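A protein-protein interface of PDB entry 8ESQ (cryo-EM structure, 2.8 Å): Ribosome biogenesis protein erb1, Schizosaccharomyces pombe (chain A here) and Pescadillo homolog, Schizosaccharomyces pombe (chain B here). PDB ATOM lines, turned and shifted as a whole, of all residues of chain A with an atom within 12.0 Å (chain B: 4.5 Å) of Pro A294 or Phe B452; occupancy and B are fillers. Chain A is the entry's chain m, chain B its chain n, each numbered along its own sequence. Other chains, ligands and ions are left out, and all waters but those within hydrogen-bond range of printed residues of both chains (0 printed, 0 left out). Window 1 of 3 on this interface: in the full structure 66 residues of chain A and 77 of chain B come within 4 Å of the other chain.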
ATOM      1  N   PRO A 289     -31.345  -4.502 -24.474  1.00  0.00           N
ATOM      2  CA  PRO A 289     -30.037  -4.488 -23.792  1.00  0.00           C
ATOM      3  C   PRO A 289     -29.447  -5.866 -23.537  1.00  0.00           C
ATOM      4  O   PRO A 289     -28.237  -5.956 -23.294  1.00  0.00           O
ATOM      5  CB  PRO A 289     -30.315  -3.755 -22.471  1.00  0.00           C
ATOM      6  CG  PRO A 289     -31.744  -3.390 -22.467  1.00  0.00           C
ATOM      7  CD  PRO A 289     -32.387  -3.758 -23.750  1.00  0.00           C
ATOM      8  N   LYS A 290     -30.247  -6.934 -23.578  1.00  0.00           N
ATOM      9  CA  LYS A 290     -29.757  -8.302 -23.397  1.00  0.00           C
ATOM     10  C   LYS A 290     -29.089  -8.488 -22.031  1.00  0.00           C
ATOM     11  O   LYS A 290     -27.867  -8.584 -21.905  1.00  0.00           O
ATOM     12  CB  LYS A 290     -28.811  -8.723 -24.522  1.00  0.00           C
ATOM     13  CG  LYS A 290     -29.497  -9.550 -25.574  1.00  0.00           C
ATOM     14  CD  LYS A 290     -28.500 -10.461 -26.237  1.00  0.00           C
ATOM     15  CE  LYS A 290     -29.185 -11.518 -27.070  1.00  0.00           C
ATOM     16  NZ  LYS A 290     -28.176 -12.410 -27.682  1.00  0.00           N
ATOM     17  N   LEU A 291     -29.944  -8.504 -21.008  1.00  0.00           N
ATOM     18  CA  LEU A 291     -29.595  -8.755 -19.613  1.00  0.00           C
ATOM     19  C   LEU A 291     -28.499  -9.808 -19.470  1.00  0.00           C
ATOM     20  O   LEU A 291     -28.502 -10.818 -20.187  1.00  0.00           O
ATOM     21  CB  LEU A 291     -30.847  -9.180 -18.842  1.00  0.00           C
ATOM     22  CG  LEU A 291     -31.753 -10.248 -19.465  1.00  0.00           C
ATOM     23  CD1 LEU A 291     -31.330 -11.657 -19.078  1.00  0.00           C
ATOM     24  CD2 LEU A 291     -33.205 -10.001 -19.082  1.00  0.00           C
ATOM     25  N   PRO A 292     -27.542  -9.596 -18.571  1.00  0.00           N
ATOM     26  CA  PRO A 292     -26.363 -10.465 -18.505  1.00  0.00           C
ATOM     27  C   PRO A 292     -26.727 -11.853 -18.011  1.00  0.00           C
ATOM     28  O   PRO A 292     -27.815 -12.054 -17.452  1.00  0.00           O
ATOM     29  CB  PRO A 292     -25.449  -9.733 -17.509  1.00  0.00           C
ATOM     30  CG  PRO A 292     -26.380  -8.980 -16.637  1.00  0.00           C
ATOM     31  CD  PRO A 292     -27.549  -8.586 -17.499  1.00  0.00           C
ATOM     32  N   PRO A 293     -25.849 -12.837 -18.205  1.00  0.00           N
ATOM     33  CA  PRO A 293     -26.183 -14.199 -17.802  1.00  0.00           C
ATOM     34  C   PRO A 293     -26.384 -14.281 -16.299  1.00  0.00           C
ATOM     35  O   PRO A 293     -25.793 -13.498 -15.533  1.00  0.00           O
ATOM     36  CB  PRO A 293     -24.962 -15.012 -18.251  1.00  0.00           C
ATOM     37  CG  PRO A 293     -23.858 -14.025 -18.340  1.00  0.00           C
ATOM     38  CD  PRO A 293     -24.502 -12.756 -18.797  1.00  0.00           C
ATOM     39  N   PRO A 294     -27.218 -15.213 -15.838  1.00  0.00           N
ATOM     40  CA  PRO A 294     -27.489 -15.311 -14.398  1.00  0.00           C
ATOM     41  C   PRO A 294     -26.286 -15.798 -13.607  1.00  0.00           C
ATOM     42  O   PRO A 294     -25.204 -16.006 -14.163  1.00  0.00           O
ATOM     43  CB  PRO A 294     -28.652 -16.312 -14.321  1.00  0.00           C
ATOM     44  CG  PRO A 294     -29.159 -16.457 -15.725  1.00  0.00           C
ATOM     45  CD  PRO A 294     -27.993 -16.192 -16.613  1.00  0.00           C
ATOM     46  N   SER A 295     -26.478 -15.982 -12.303  1.00  0.00           N
ATOM     47  CA  SER A 295     -25.381 -16.346 -11.420  1.00  0.00           C
ATOM     48  C   SER A 295     -24.781 -17.689 -11.820  1.00  0.00           C
ATOM     49  O   SER A 295     -25.473 -18.587 -12.305  1.00  0.00           O
ATOM     50  CB  SER A 295     -25.872 -16.391  -9.977  1.00  0.00           C
ATOM     51  OG  SER A 295     -26.506 -15.175  -9.624  1.00  0.00           O
ATOM     52  N   HIS A 296     -23.472 -17.817 -11.609  1.00  0.00           N
ATOM     53  CA  HIS A 296     -22.684 -18.914 -12.155  1.00  0.00           C
ATOM     54  C   HIS A 296     -22.378 -20.009 -11.141  1.00  0.00           C
ATOM     55  O   HIS A 296     -21.511 -20.847 -11.406  1.00  0.00           O
ATOM     56  CB  HIS A 296     -21.378 -18.372 -12.739  1.00  0.00           C
ATOM     57  CG  HIS A 296     -20.736 -17.313 -11.899  1.00  0.00           C
ATOM     58  ND1 HIS A 296     -19.843 -17.602 -10.890  1.00  0.00           N
ATOM     59  CD2 HIS A 296     -20.859 -15.965 -11.916  1.00  0.00           C
ATOM     60  CE1 HIS A 296     -19.443 -16.478 -10.323  1.00  0.00           C
ATOM     61  NE2 HIS A 296     -20.044 -15.469 -10.927  1.00  0.00           N
ATOM     62  N   GLU A 297     -23.072 -20.025  -9.999  1.00  0.00           N
ATOM     63  CA  GLU A 297     -22.875 -21.029  -8.947  1.00  0.00           C
ATOM     64  C   GLU A 297     -21.523 -20.868  -8.250  1.00  0.00           C
ATOM     65  O   GLU A 297     -20.778 -21.831  -8.072  1.00  0.00           O
ATOM     66  CB  GLU A 297     -23.043 -22.452  -9.494  1.00  0.00           C
ATOM     67  CG  GLU A 297     -23.351 -23.507  -8.452  1.00  0.00           C
ATOM     68  CD  GLU A 297     -23.663 -24.848  -9.076  1.00  0.00           C
ATOM     69  OE1 GLU A 297     -23.876 -24.897 -10.305  1.00  0.00           O
ATOM     70  OE2 GLU A 297     -23.686 -25.855  -8.342  1.00  0.00           O
ATOM     71  N   GLU A 298     -21.200 -19.635  -7.863  1.00  0.00           N
ATOM     72  CA  GLU A 298     -20.070 -19.345  -6.987  1.00  0.00           C
ATOM     73  C   GLU A 298     -20.576 -18.502  -5.826  1.00  0.00           C
ATOM     74  O   GLU A 298     -21.123 -17.415  -6.038  1.00  0.00           O
ATOM     75  CB  GLU A 298     -18.951 -18.626  -7.741  1.00  0.00           C
ATOM     76  CG  GLU A 298     -17.915 -19.565  -8.338  1.00  0.00           C
ATOM     77  CD  GLU A 298     -18.377 -20.224  -9.614  1.00  0.00           C
ATOM     78  OE1 GLU A 298     -19.438 -19.830 -10.130  1.00  0.00           O
ATOM     79  OE2 GLU A 298     -17.683 -21.142 -10.097  1.00  0.00           O
ATOM     80  N   SER A 299     -20.390 -18.998  -4.608  1.00  0.00           N
ATOM     81  CA  SER A 299     -21.023 -18.414  -3.431  1.00  0.00           C
ATOM     82  C   SER A 299     -20.140 -18.647  -2.212  1.00  0.00           C
ATOM     83  O   SER A 299     -18.929 -18.861  -2.335  1.00  0.00           O
ATOM     84  CB  SER A 299     -22.433 -18.986  -3.233  1.00  0.00           C
ATOM     85  OG  SER A 299     -23.355 -18.310  -4.055  1.00  0.00           O
ATOM     86  N   TYR A 300     -20.751 -18.555  -1.029  1.00  0.00           N
ATOM     87  CA  TYR A 300     -20.059 -18.766   0.237  1.00  0.00           C
ATOM     88  C   TYR A 300     -19.361 -20.116   0.266  1.00  0.00           C
ATOM     89  O   TYR A 300     -18.152 -20.207   0.495  1.00  0.00           O
ATOM     90  CB  TYR A 300     -21.056 -18.688   1.399  1.00  0.00           C
ATOM     91  CG  TYR A 300     -21.943 -17.469   1.426  1.00  0.00           C
ATOM     92  CD1 TYR A 300     -21.645 -16.340   0.675  1.00  0.00           C
ATOM     93  CD2 TYR A 300     -23.092 -17.454   2.203  1.00  0.00           C
ATOM     94  CE1 TYR A 300     -22.460 -15.231   0.700  1.00  0.00           C
ATOM     95  CE2 TYR A 300     -23.912 -16.348   2.236  1.00  0.00           C
ATOM     96  CZ  TYR A 300     -23.593 -15.239   1.483  1.00  0.00           C
ATOM     97  OH  TYR A 300     -24.408 -14.133   1.506  1.00  0.00           O
ATOM     98  N   GLU A 304     -18.550 -26.178  -6.854  1.00  0.00           N
ATOM     99  CA  GLU A 304     -18.278 -26.178  -8.286  1.00  0.00           C
ATOM    100  C   GLU A 304     -16.797 -25.965  -8.572  1.00  0.00           C
ATOM    101  O   GLU A 304     -16.231 -26.608  -9.463  1.00  0.00           O
ATOM    102  CB  GLU A 304     -19.119 -25.103  -8.972  1.00  0.00           C
ATOM    103  CG  GLU A 304     -19.049 -25.128 -10.487  1.00  0.00           C
ATOM    104  CD  GLU A 304     -19.064 -26.537 -11.042  1.00  0.00           C
ATOM    105  OE1 GLU A 304     -20.117 -27.202 -10.947  1.00  0.00           O
ATOM    106  OE2 GLU A 304     -18.026 -26.979 -11.579  1.00  0.00           O
ATOM    107  N   LYS A 333     -21.286  -2.557 -11.892  1.00  0.00           N
ATOM    108  CA  LYS A 333     -22.499  -1.853 -12.294  1.00  0.00           C
ATOM    109  C   LYS A 333     -22.171  -0.609 -13.105  1.00  0.00           C
ATOM    110  O   LYS A 333     -22.933  -0.230 -14.002  1.00  0.00           O
ATOM    111  CB  LYS A 333     -23.330  -1.490 -11.068  1.00  0.00           C
ATOM    112  CG  LYS A 333     -23.688  -2.678 -10.205  1.00  0.00           C
ATOM    113  CD  LYS A 333     -24.361  -3.761 -11.019  1.00  0.00           C
ATOM    114  CE  LYS A 333     -24.771  -4.915 -10.133  1.00  0.00           C
ATOM    115  NZ  LYS A 333     -25.738  -4.461  -9.100  1.00  0.00           N
ATOM    116  N   ARG A 336     -21.552  -1.912 -16.439  1.00  0.00           N
ATOM    117  CA  ARG A 336     -22.841  -2.247 -17.031  1.00  0.00           C
ATOM    118  C   ARG A 336     -23.527  -1.003 -17.575  1.00  0.00           C
ATOM    119  O   ARG A 336     -24.073  -1.014 -18.684  1.00  0.00           O
ATOM    120  CB  ARG A 336     -23.729  -2.942 -16.002  1.00  0.00           C
ATOM    121  CG  ARG A 336     -25.117  -3.244 -16.513  1.00  0.00           C
ATOM    122  CD  ARG A 336     -25.064  -4.272 -17.623  1.00  0.00           C
ATOM    123  NE  ARG A 336     -26.386  -4.785 -17.955  1.00  0.00           N
ATOM    124  CZ  ARG A 336     -26.757  -5.159 -19.169  1.00  0.00           C
ATOM    125  NH1 ARG A 336     -25.927  -5.089 -20.196  1.00  0.00           N
ATOM    126  NH2 ARG A 336     -27.991  -5.615 -19.359  1.00  0.00           N
ATOM    127  N   LYS B 179     -36.812 -17.082  -6.217  1.00  0.00           N
ATOM    128  CA  LYS B 179     -35.511 -17.628  -5.867  1.00  0.00           C
ATOM    129  C   LYS B 179     -34.666 -16.557  -5.193  1.00  0.00           C
ATOM    130  O   LYS B 179     -34.782 -15.368  -5.498  1.00  0.00           O
ATOM    131  CB  LYS B 179     -34.800 -18.177  -7.114  1.00  0.00           C
ATOM    132  CG  LYS B 179     -35.569 -19.304  -7.796  1.00  0.00           C
ATOM    133  CD  LYS B 179     -34.817 -19.900  -8.970  1.00  0.00           C
ATOM    134  CE  LYS B 179     -34.939 -19.043 -10.214  1.00  0.00           C
ATOM    135  NZ  LYS B 179     -34.312 -19.700 -11.393  1.00  0.00           N
ATOM    136  N   PHE B 181     -30.514 -16.146  -3.866  1.00  0.00           N
ATOM    137  CA  PHE B 181     -29.208 -16.776  -4.009  1.00  0.00           C
ATOM    138  C   PHE B 181     -28.160 -15.921  -3.315  1.00  0.00           C
ATOM    139  O   PHE B 181     -27.923 -14.779  -3.720  1.00  0.00           O
ATOM    140  CB  PHE B 181     -28.874 -16.958  -5.490  1.00  0.00           C
ATOM    141  CG  PHE B 181     -27.535 -17.572  -5.750  1.00  0.00           C
ATOM    142  CD1 PHE B 181     -27.197 -18.793  -5.197  1.00  0.00           C
ATOM    143  CD2 PHE B 181     -26.625 -16.946  -6.579  1.00  0.00           C
ATOM    144  CE1 PHE B 181     -25.971 -19.364  -5.451  1.00  0.00           C
ATOM    145  CE2 PHE B 181     -25.399 -17.513  -6.832  1.00  0.00           C
ATOM    146  CZ  PHE B 181     -25.076 -18.725  -6.279  1.00  0.00           C
ATOM    147  N   TYR B 188     -28.833 -12.426  -4.785  1.00  0.00           N
ATOM    148  CA  TYR B 188     -29.540 -12.428  -6.060  1.00  0.00           C
ATOM    149  C   TYR B 188     -30.983 -12.846  -5.817  1.00  0.00           C
ATOM    150  O   TYR B 188     -31.253 -14.007  -5.497  1.00  0.00           O
ATOM    151  CB  TYR B 188     -28.871 -13.371  -7.053  1.00  0.00           C
ATOM    152  CG  TYR B 188     -27.616 -12.830  -7.687  1.00  0.00           C
ATOM    153  CD1 TYR B 188     -26.391 -12.936  -7.047  1.00  0.00           C
ATOM    154  CD2 TYR B 188     -27.654 -12.229  -8.936  1.00  0.00           C
ATOM    155  CE1 TYR B 188     -25.240 -12.449  -7.629  1.00  0.00           C
ATOM    156  CE2 TYR B 188     -26.509 -11.739  -9.525  1.00  0.00           C
ATOM    157  CZ  TYR B 188     -25.306 -11.852  -8.867  1.00  0.00           C
ATOM    158  OH  TYR B 188     -24.160 -11.365  -9.450  1.00  0.00           O
ATOM    159  N   GLN B 190     -34.934 -13.244  -7.368  1.00  0.00           N
ATOM    160  CA  GLN B 190     -35.542 -13.599  -8.648  1.00  0.00           C
ATOM    161  C   GLN B 190     -37.040 -13.733  -8.408  1.00  0.00           C
ATOM    162  O   GLN B 190     -37.488 -14.688  -7.767  1.00  0.00           O
ATOM    163  CB  GLN B 190     -34.945 -14.885  -9.200  1.00  0.00           C
ATOM    164  CG  GLN B 190     -35.798 -15.580 -10.238  1.00  0.00           C
ATOM    165  CD  GLN B 190     -35.528 -15.077 -11.634  1.00  0.00           C
ATOM    166  OE1 GLN B 190     -34.376 -14.965 -12.054  1.00  0.00           O
ATOM    167  NE2 GLN B 190     -36.588 -14.769 -12.365  1.00  0.00           N
ATOM    168  N   SER B 450     -26.708 -22.809  -6.968  1.00  0.00           N
ATOM    169  CA  SER B 450     -27.262 -21.692  -7.716  1.00  0.00           C
ATOM    170  C   SER B 450     -28.630 -22.076  -8.258  1.00  0.00           C
ATOM    171  O   SER B 450     -28.720 -22.977  -9.099  1.00  0.00           O
ATOM    172  CB  SER B 450     -26.346 -21.301  -8.863  1.00  0.00           C
ATOM    173  OG  SER B 450     -26.999 -20.417  -9.756  1.00  0.00           O
ATOM    174  N   PRO B 451     -29.710 -21.429  -7.815  1.00  0.00           N
ATOM    175  CA  PRO B 451     -31.024 -21.703  -8.406  1.00  0.00           C
ATOM    176  C   PRO B 451     -31.182 -21.153  -9.812  1.00  0.00           C
ATOM    177  O   PRO B 451     -32.260 -21.298 -10.399  1.00  0.00           O
ATOM    178  CB  PRO B 451     -31.987 -21.022  -7.426  1.00  0.00           C
ATOM    179  CG  PRO B 451     -31.191 -19.925  -6.831  1.00  0.00           C
ATOM    180  CD  PRO B 451     -29.785 -20.439  -6.730  1.00  0.00           C
ATOM    181  N   PHE B 452     -30.138 -20.534 -10.370  1.00  0.00           N
ATOM    182  CA  PHE B 452     -30.169 -20.014 -11.727  1.00  0.00           C
ATOM    183  C   PHE B 452     -29.402 -20.868 -12.722  1.00  0.00           C
ATOM    184  O   PHE B 452     -29.718 -20.828 -13.914  1.00  0.00           O
ATOM    185  CB  PHE B 452     -29.595 -18.591 -11.766  1.00  0.00           C
ATOM    186  CG  PHE B 452     -30.169 -17.680 -10.728  1.00  0.00           C
ATOM    187  CD1 PHE B 452     -31.482 -17.260 -10.808  1.00  0.00           C
ATOM    188  CD2 PHE B 452     -29.391 -17.237  -9.675  1.00  0.00           C
ATOM    189  CE1 PHE B 452     -32.009 -16.423  -9.855  1.00  0.00           C
ATOM    190  CE2 PHE B 452     -29.916 -16.396  -8.721  1.00  0.00           C
ATOM    191  CZ  PHE B 452     -31.226 -15.990  -8.810  1.00  0.00           C
ATOM    192  N   VAL B 453     -28.412 -21.629 -12.270  1.00  0.00           N
ATOM    193  CA  VAL B 453     -27.630 -22.471 -13.166  1.00  0.00           C
ATOM    194  C   VAL B 453     -28.476 -23.666 -13.580  1.00  0.00           C
ATOM    195  O   VAL B 453     -28.973 -24.416 -12.732  1.00  0.00           O
ATOM    196  CB  VAL B 453     -26.326 -22.923 -12.490  1.00  0.00           C
ATOM    197  CG1 VAL B 453     -25.724 -24.104 -13.233  1.00  0.00           C
ATOM    198  CG2 VAL B 453     -25.337 -21.774 -12.427  1.00  0.00           C
ATOM    199  N   LYS B 454     -28.645 -23.842 -14.886  1.00  0.00           N
ATOM    200  CA  LYS B 454     -29.369 -24.977 -15.433  1.00  0.00           C
ATOM    201  C   LYS B 454     -28.385 -26.083 -15.783  1.00  0.00           C
ATOM    202  O   LYS B 454     -27.309 -25.820 -16.329  1.00  0.00           O
ATOM    203  CB  LYS B 454     -30.174 -24.576 -16.669  1.00  0.00           C
ATOM    204  CG  LYS B 454     -31.376 -23.697 -16.364  1.00  0.00           C
ATOM    205  CD  LYS B 454     -32.275 -24.331 -15.313  1.00  0.00           C
ATOM    206  CE  LYS B 454     -32.880 -25.635 -15.808  1.00  0.00           C
ATOM    207  NZ  LYS B 454     -33.785 -26.244 -14.794  1.00  0.00           N
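The side-chain hydroxyl of Ser B450 sits at hydrogen-bond distance from the backbone carbonyl oxygen of Ser A295.
The backbone carbonyl oxygen of His A296 lies close to the side-chain carboxylate of Glu A298. N of Tyr B188 is in hydrogen-bond range of O of Phe B181. N of Phe B452 lies close to OG of Ser B450 (3.2 Å). The side-chain hydroxyl (OG) of Ser B450 sits at hydrogen-bond distance from the backbone NH (N) of Val B453, 3.1 Å away.
Among the printed residues, pairs that only touch across the chains: Pro A294 with Phe B452, Ser A295 with Phe B181, Ser A295 with Tyr B188, Ser A295 with Phe B452, Ser A295 with Val B453, His A296 with Val B453, Glu A297 with Ser B450, Glu A297 with Val B453 and Ser A299 with Phe B181.
Of chain B, only Phe B452 (3.6 Å) comes within 4 Å of Pro A294. Of the printed residues of chain B, Glu A297 touches Ser B450 and Val B453. Of the printed residues of chain B, Ser A299 touches Phe B181 (2.8 Å). Arg A336 touches none of the printed residues of chain B. No residue of chain A comes within 4 Å of Lys B179. Phe B181 touches two residues of chain A. No residue of chain A comes within 4 Å of Gln B190. Of chain A, only Ser A295 and Glu A297 come within 4 Å of Ser B450. Phe B452 touches just these residues of chain A: Pro A294 and Ser A295. Lys B454 touches none of the printed residues of chain A. The nearest printed residue of chain B that does not touch Pro A294 is Val B453 (5.7 Å). The nearest residue of chain A that does not touch Phe B452 is His A296 (6.2 Å). The nearest printed residue of chain B that does not touch Glu A297 is Phe B181 (4.2 Å).
Of the 15 printed residues of chain A, 5 touch a printed residue of chain B. Hydrophobic or aromatic side chains of chain A within 4 Å of the printed part of chain B: Pro A294. Of the 9 printed residues of chain B, 5 touch a printed residue of chain A. Hydrophobic or aromatic side chains of chain B within 4 Å of the printed part of chain A: Phe B181, Tyr B188, Phe B452 and Val B453. Among the printed residues, 10 pairs touch across the chains. Among the printed residues, no Asp or Glu carboxylate lies within 4 Å of a Lys or Arg side-chain nitrogen of the other chain.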
